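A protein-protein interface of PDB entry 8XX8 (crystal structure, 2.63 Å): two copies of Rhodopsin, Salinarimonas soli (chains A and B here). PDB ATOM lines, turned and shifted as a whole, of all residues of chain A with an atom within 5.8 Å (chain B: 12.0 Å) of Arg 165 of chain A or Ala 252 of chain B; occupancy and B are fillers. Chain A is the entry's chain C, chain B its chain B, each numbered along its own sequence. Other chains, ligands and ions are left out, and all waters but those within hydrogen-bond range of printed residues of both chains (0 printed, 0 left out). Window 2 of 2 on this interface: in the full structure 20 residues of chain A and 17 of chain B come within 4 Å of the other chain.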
ATOM      1  N   ALA A  99      -1.308  -7.427   7.129  1.00  0.00           N
ATOM      2  CA  ALA A  99      -0.951  -8.467   6.174  1.00  0.00           C
ATOM      3  C   ALA A  99       0.410  -8.227   5.537  1.00  0.00           C
ATOM      4  O   ALA A  99       1.093  -9.190   5.170  1.00  0.00           O
ATOM      5  CB  ALA A  99      -2.022  -8.567   5.086  1.00  0.00           C
ATOM      6  N   LEU A 160      -4.849 -10.101  -0.261  1.00  0.00           N
ATOM      7  CA  LEU A 160      -4.347  -9.645   1.030  1.00  0.00           C
ATOM      8  C   LEU A 160      -4.200 -10.807   2.005  1.00  0.00           C
ATOM      9  O   LEU A 160      -3.226 -10.869   2.765  1.00  0.00           O
ATOM     10  CB  LEU A 160      -5.277  -8.575   1.600  1.00  0.00           C
ATOM     11  CG  LEU A 160      -4.653  -7.285   2.123  1.00  0.00           C
ATOM     12  CD1 LEU A 160      -3.759  -6.659   1.068  1.00  0.00           C
ATOM     13  CD2 LEU A 160      -5.748  -6.316   2.538  1.00  0.00           C
ATOM     14  N   LEU A 161      -5.157 -11.739   1.995  1.00  0.00           N
ATOM     15  CA  LEU A 161      -5.041 -12.931   2.830  1.00  0.00           C
ATOM     16  C   LEU A 161      -3.881 -13.808   2.376  1.00  0.00           C
ATOM     17  O   LEU A 161      -3.157 -14.371   3.205  1.00  0.00           O
ATOM     18  CB  LEU A 161      -6.353 -13.717   2.809  1.00  0.00           C
ATOM     19  CG  LEU A 161      -6.335 -15.098   3.471  1.00  0.00           C
ATOM     20  CD1 LEU A 161      -5.954 -14.988   4.939  1.00  0.00           C
ATOM     21  CD2 LEU A 161      -7.681 -15.785   3.311  1.00  0.00           C
ATOM     22  N   LEU A 162      -3.693 -13.940   1.060  1.00  0.00           N
ATOM     23  CA  LEU A 162      -2.537 -14.670   0.550  1.00  0.00           C
ATOM     24  C   LEU A 162      -1.233 -13.993   0.946  1.00  0.00           C
ATOM     25  O   LEU A 162      -0.218 -14.671   1.145  1.00  0.00           O
ATOM     26  CB  LEU A 162      -2.627 -14.800  -0.971  1.00  0.00           C
ATOM     27  CG  LEU A 162      -3.197 -16.097  -1.552  1.00  0.00           C
ATOM     28  CD1 LEU A 162      -4.506 -16.479  -0.881  1.00  0.00           C
ATOM     29  CD2 LEU A 162      -3.385 -15.954  -3.055  1.00  0.00           C
ATOM     30  N   GLU A 163      -1.238 -12.664   1.065  1.00  0.00           N
ATOM     31  CA  GLU A 163      -0.035 -11.944   1.464  1.00  0.00           C
ATOM     32  C   GLU A 163       0.194 -11.992   2.969  1.00  0.00           C
ATOM     33  O   GLU A 163       1.338 -11.873   3.420  1.00  0.00           O
ATOM     34  CB  GLU A 163      -0.112 -10.489   0.997  1.00  0.00           C
ATOM     35  CG  GLU A 163       0.103 -10.294  -0.494  1.00  0.00           C
ATOM     36  CD  GLU A 163       1.526 -10.592  -0.928  1.00  0.00           C
ATOM     37  OE1 GLU A 163       1.751 -10.782  -2.140  1.00  0.00           O
ATOM     38  OE2 GLU A 163       2.424 -10.635  -0.061  1.00  0.00           O
ATOM     39  N   ALA A 164      -0.871 -12.164   3.755  1.00  0.00           N
ATOM     40  CA  ALA A 164      -0.721 -12.214   5.206  1.00  0.00           C
ATOM     41  C   ALA A 164       0.103 -13.422   5.640  1.00  0.00           C
ATOM     42  O   ALA A 164       0.970 -13.307   6.513  1.00  0.00           O
ATOM     43  CB  ALA A 164      -2.095 -12.228   5.875  1.00  0.00           C
ATOM     44  N   ARG A 165      -0.153 -14.589   5.043  1.00  0.00           N
ATOM     45  CA  ARG A 165       0.614 -15.780   5.393  1.00  0.00           C
ATOM     46  C   ARG A 165       2.070 -15.685   4.956  1.00  0.00           C
ATOM     47  O   ARG A 165       2.923 -16.368   5.533  1.00  0.00           O
ATOM     48  CB  ARG A 165      -0.034 -17.028   4.787  1.00  0.00           C
ATOM     49  CG  ARG A 165      -0.624 -16.820   3.403  1.00  0.00           C
ATOM     50  CD  ARG A 165      -0.913 -18.146   2.711  1.00  0.00           C
ATOM     51  NE  ARG A 165       0.313 -18.844   2.332  1.00  0.00           N
ATOM     52  CZ  ARG A 165       0.349 -19.992   1.664  1.00  0.00           C
ATOM     53  NH1 ARG A 165      -0.777 -20.585   1.292  1.00  0.00           N
ATOM     54  NH2 ARG A 165       1.515 -20.549   1.365  1.00  0.00           N
ATOM     55  N   VAL A 166       2.375 -14.860   3.952  1.00  0.00           N
ATOM     56  CA  VAL A 166       3.764 -14.677   3.540  1.00  0.00           C
ATOM     57  C   VAL A 166       4.525 -13.863   4.580  1.00  0.00           C
ATOM     58  O   VAL A 166       5.709 -14.113   4.839  1.00  0.00           O
ATOM     59  CB  VAL A 166       3.824 -14.022   2.148  1.00  0.00           C
ATOM     60  CG1 VAL A 166       5.267 -13.829   1.709  1.00  0.00           C
ATOM     61  CG2 VAL A 166       3.065 -14.860   1.134  1.00  0.00           C
ATOM     62  N   THR A 167       3.858 -12.883   5.196  1.00  0.00           N
ATOM     63  CA  THR A 167       4.516 -12.048   6.197  1.00  0.00           C
ATOM     64  C   THR A 167       4.935 -12.865   7.414  1.00  0.00           C
ATOM     65  O   THR A 167       6.032 -12.672   7.953  1.00  0.00           O
ATOM     66  CB  THR A 167       3.591 -10.905   6.614  1.00  0.00           C
ATOM     67  OG1 THR A 167       3.215 -10.149   5.458  1.00  0.00           O
ATOM     68  CG2 THR A 167       4.290  -9.989   7.609  1.00  0.00           C
ATOM     69  N   GLY A 168       4.084 -13.777   7.856  1.00  0.00           N
ATOM     70  CA  GLY A 168       4.402 -14.608   8.999  1.00  0.00           C
ATOM     71  C   GLY A 168       3.153 -15.210   9.596  1.00  0.00           C
ATOM     72  O   GLY A 168       2.030 -14.805   9.302  1.00  0.00           O
ATOM     73  N   ALA A 169       3.376 -16.205  10.460  1.00  0.00           N
ATOM     74  CA  ALA A 169       2.257 -16.883  11.105  1.00  0.00           C
ATOM     75  C   ALA A 169       1.527 -15.955  12.069  1.00  0.00           C
ATOM     76  O   ALA A 169       0.297 -16.005  12.174  1.00  0.00           O
ATOM     77  CB  ALA A 169       2.750 -18.135  11.828  1.00  0.00           C
ATOM     78  N   ARG A 172      -0.478 -13.553  10.080  1.00  0.00           N
ATOM     79  CA  ARG A 172      -1.598 -14.247   9.451  1.00  0.00           C
ATOM     80  C   ARG A 172      -2.760 -14.405  10.422  1.00  0.00           C
ATOM     81  O   ARG A 172      -3.915 -14.134  10.072  1.00  0.00           O
ATOM     82  CB  ARG A 172      -1.148 -15.611   8.930  1.00  0.00           C
ATOM     83  CG  ARG A 172      -2.246 -16.378   8.213  1.00  0.00           C
ATOM     84  CD  ARG A 172      -1.889 -17.843   8.030  1.00  0.00           C
ATOM     85  NE  ARG A 172      -2.894 -18.543   7.234  1.00  0.00           N
ATOM     86  CZ  ARG A 172      -4.037 -19.016   7.720  1.00  0.00           C
ATOM     87  NH1 ARG A 172      -4.325 -18.867   9.007  1.00  0.00           N
ATOM     88  NH2 ARG A 172      -4.893 -19.638   6.921  1.00  0.00           N
ATOM     89  N   LEU B 243       4.529 -16.378 -13.601  1.00  0.00           N
ATOM     90  CA  LEU B 243       3.662 -16.402 -12.434  1.00  0.00           C
ATOM     91  C   LEU B 243       3.088 -15.018 -12.168  1.00  0.00           C
ATOM     92  O   LEU B 243       3.790 -14.010 -12.288  1.00  0.00           O
ATOM     93  CB  LEU B 243       4.432 -16.873 -11.200  1.00  0.00           C
ATOM     94  CG  LEU B 243       4.173 -18.278 -10.663  1.00  0.00           C
ATOM     95  CD1 LEU B 243       4.339 -19.317 -11.757  1.00  0.00           C
ATOM     96  CD2 LEU B 243       5.124 -18.550  -9.516  1.00  0.00           C
ATOM     97  N   THR B 244       1.812 -14.973 -11.795  1.00  0.00           N
ATOM     98  CA  THR B 244       1.240 -13.728 -11.316  1.00  0.00           C
ATOM     99  C   THR B 244       1.679 -13.476  -9.877  1.00  0.00           C
ATOM    100  O   THR B 244       2.176 -14.369  -9.187  1.00  0.00           O
ATOM    101  CB  THR B 244      -0.288 -13.748 -11.401  1.00  0.00           C
ATOM    102  OG1 THR B 244      -0.810 -14.707 -10.474  1.00  0.00           O
ATOM    103  CG2 THR B 244      -0.743 -14.101 -12.809  1.00  0.00           C
ATOM    104  N   LEU B 245       1.492 -12.232  -9.427  1.00  0.00           N
ATOM    105  CA  LEU B 245       1.904 -11.880  -8.071  1.00  0.00           C
ATOM    106  C   LEU B 245       1.086 -12.622  -7.022  1.00  0.00           C
ATOM    107  O   LEU B 245       1.607 -12.939  -5.946  1.00  0.00           O
ATOM    108  CB  LEU B 245       1.803 -10.368  -7.865  1.00  0.00           C
ATOM    109  CG  LEU B 245       2.796  -9.541  -8.686  1.00  0.00           C
ATOM    110  CD1 LEU B 245       2.592  -8.057  -8.449  1.00  0.00           C
ATOM    111  CD2 LEU B 245       4.225  -9.944  -8.359  1.00  0.00           C
ATOM    112  N   ASP B 246      -0.186 -12.913  -7.312  1.00  0.00           N
ATOM    113  CA  ASP B 246      -0.989 -13.708  -6.388  1.00  0.00           C
ATOM    114  C   ASP B 246      -0.537 -15.162  -6.376  1.00  0.00           C
ATOM    115  O   ASP B 246      -0.492 -15.795  -5.314  1.00  0.00           O
ATOM    116  CB  ASP B 246      -2.469 -13.608  -6.754  1.00  0.00           C
ATOM    117  CG  ASP B 246      -3.074 -12.275  -6.368  1.00  0.00           C
ATOM    118  OD1 ASP B 246      -2.575 -11.658  -5.404  1.00  0.00           O
ATOM    119  OD2 ASP B 246      -4.047 -11.846  -7.022  1.00  0.00           O
ATOM    120  N   GLU B 247      -0.199 -15.710  -7.546  1.00  0.00           N
ATOM    121  CA  GLU B 247       0.311 -17.075  -7.604  1.00  0.00           C
ATOM    122  C   GLU B 247       1.639 -17.196  -6.868  1.00  0.00           C
ATOM    123  O   GLU B 247       1.918 -18.220  -6.236  1.00  0.00           O
ATOM    124  CB  GLU B 247       0.456 -17.522  -9.058  1.00  0.00           C
ATOM    125  CG  GLU B 247      -0.868 -17.764  -9.766  1.00  0.00           C
ATOM    126  CD  GLU B 247      -0.727 -17.815 -11.276  1.00  0.00           C
ATOM    127  OE1 GLU B 247       0.363 -17.483 -11.786  1.00  0.00           O
ATOM    128  OE2 GLU B 247      -1.708 -18.186 -11.955  1.00  0.00           O
ATOM    129  N   ALA B 248       2.470 -16.153  -6.936  1.00  0.00           N
ATOM    130  CA  ALA B 248       3.722 -16.160  -6.190  1.00  0.00           C
ATOM    131  C   ALA B 248       3.477 -16.076  -4.689  1.00  0.00           C
ATOM    132  O   ALA B 248       4.224 -16.673  -3.904  1.00  0.00           O
ATOM    133  CB  ALA B 248       4.616 -15.007  -6.649  1.00  0.00           C
ATOM    134  N   ALA B 249       2.437 -15.349  -4.275  1.00  0.00           N
ATOM    135  CA  ALA B 249       2.128 -15.236  -2.853  1.00  0.00           C
ATOM    136  C   ALA B 249       1.622 -16.560  -2.290  1.00  0.00           C
ATOM    137  O   ALA B 249       1.936 -16.913  -1.147  1.00  0.00           O
ATOM    138  CB  ALA B 249       1.102 -14.127  -2.622  1.00  0.00           C
ATOM    139  N   ARG B 250       0.841 -17.305  -3.075  1.00  0.00           N
ATOM    140  CA  ARG B 250       0.342 -18.593  -2.604  1.00  0.00           C
ATOM    141  C   ARG B 250       1.479 -19.586  -2.402  1.00  0.00           C
ATOM    142  O   ARG B 250       1.487 -20.339  -1.420  1.00  0.00           O
ATOM    143  CB  ARG B 250      -0.694 -19.148  -3.582  1.00  0.00           C
ATOM    144  CG  ARG B 250      -1.147 -20.562  -3.253  1.00  0.00           C
ATOM    145  CD  ARG B 250      -2.393 -20.949  -4.028  1.00  0.00           C
ATOM    146  NE  ARG B 250      -3.550 -20.147  -3.639  1.00  0.00           N
ATOM    147  CZ  ARG B 250      -4.318 -20.406  -2.586  1.00  0.00           C
ATOM    148  NH1 ARG B 250      -4.051 -21.448  -1.807  1.00  0.00           N
ATOM    149  NH2 ARG B 250      -5.352 -19.625  -2.306  1.00  0.00           N
ATOM    150  N   ARG B 251       2.454 -19.599  -3.314  1.00  0.00           N
ATOM    151  CA  ARG B 251       3.571 -20.527  -3.182  1.00  0.00           C
ATOM    152  C   ARG B 251       4.508 -20.126  -2.050  1.00  0.00           C
ATOM    153  O   ARG B 251       5.166 -20.989  -1.457  1.00  0.00           O
ATOM    154  CB  ARG B 251       4.339 -20.615  -4.502  1.00  0.00           C
ATOM    155  CG  ARG B 251       3.474 -20.998  -5.690  1.00  0.00           C
ATOM    156  CD  ARG B 251       4.222 -20.793  -6.993  1.00  0.00           C
ATOM    157  NE  ARG B 251       4.938 -21.987  -7.429  1.00  0.00           N
ATOM    158  CZ  ARG B 251       4.642 -22.672  -8.528  1.00  0.00           C
ATOM    159  NH1 ARG B 251       3.646 -22.276  -9.310  1.00  0.00           N
ATOM    160  NH2 ARG B 251       5.345 -23.749  -8.852  1.00  0.00           N
ATOM    161  N   ALA B 252       4.582 -18.837  -1.734  1.00  0.00           N
ATOM    162  CA  ALA B 252       5.449 -18.360  -0.664  1.00  0.00           C
ATOM    163  C   ALA B 252       4.651 -18.068   0.603  1.00  0.00           C
ATOM    164  O   ALA B 252       3.949 -18.936   1.121  1.00  0.00           O
ATOM    165  CB  ALA B 252       6.205 -17.120  -1.111  1.00  0.00           C
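O of Arg 250 of chain B sits at hydrogen-bond distance from NH2 of Arg 165 of chain A (2.8 Å). The backbone carbonyl oxygen of Ala 252 of chain B is in hydrogen-bond range of the guanidinium group of Arg 165 of chain A (2.9 Å).
No position is printed for both chains.
The backbone carbonyl oxygen (O) of Glu 163 of chain A sits at hydrogen-bond distance from the side-chain hydroxyl (OG1) of Thr 167 of chain A (3.3 Å).
Of the 10 printed residues of chain B, 4 touch a printed residue of chain A. Printed residues of chain B that touch a printed residue of chain A: Asp 246, Ala 249, Arg 250 and Ala 252. Printed residues of chain A that touch a printed residue of chain B: Leu 162, Glu 163, Arg 165 and Val 166. Hydrophobic or aromatic side chains of chain A within 4 Å of the printed part of chain B: Leu 162 and Val 166. Among the printed residues, no Asp or Glu carboxylate lies within 4 Å of a Lys or Arg side-chain nitrogen of the other chain.
Among the printed residues, pairs that only touch across the chains: Leu 162 of chain A with Asp 246 of chain B (3.7 Å), Leu 162 of chain A with Ala 249 of chain B (3.9 Å), Leu 162 of chain A with Arg 250 of chain B (3.6 Å), Glu 163 of chain A with Ala 249 of chain B (3.4 Å), Val 166 of chain A with Ala 249 of chain B (3.3 Å) and Val 166 of chain A with Ala 252 of chain B (3.6 Å).
Arg 165 of chain A touches just these residues of chain B: Arg 250 and Ala 252. Ala 252 of chain B touches just these residues of chain A: Arg 165 (2.9 Å) and Val 166 (3.6 Å). Leu 162 of chain A touches just these residues of chain B: Asp 246, Ala 249 and Arg 250. No residue of chain B comes within 4 Å of Ala 164 of chain A. Val 166 of chain A touches two residues of chain B. No residue of chain B comes within 4 Å of Thr 167 of chain A. No residue of chain B comes within 4 Å of Ala 169 of chain A. No residue of chain B comes within 4 Å of Arg 172 of chain A. Printed residues of chain A within 4 Å of Arg 250 of chain B: Leu 162 and Arg 165. Printed residues of chain A within 4 Å of Asp 246 of chain B: Leu 162 (3.7 Å). Printed residues of chain A within 4 Å of Ala 249 of chain B: Leu 162 (3.9 Å), Glu 163 (3.4 Å) and Val 166 (3.3 Å). Thr 244 of chain B touches none of the printed residues of chain A. The nearest residue of chain B that does not touch Arg 165 of chain A is Ala 249 of chain B (4.3 Å). The nearest printed residue of chain A that does not touch Ala 252 of chain B is Leu 162 of chain A (6.0 Å). The nearest printed residue of chain A that does not touch Ala 249 of chain B is Arg 165 of chain A (4.3 Å).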
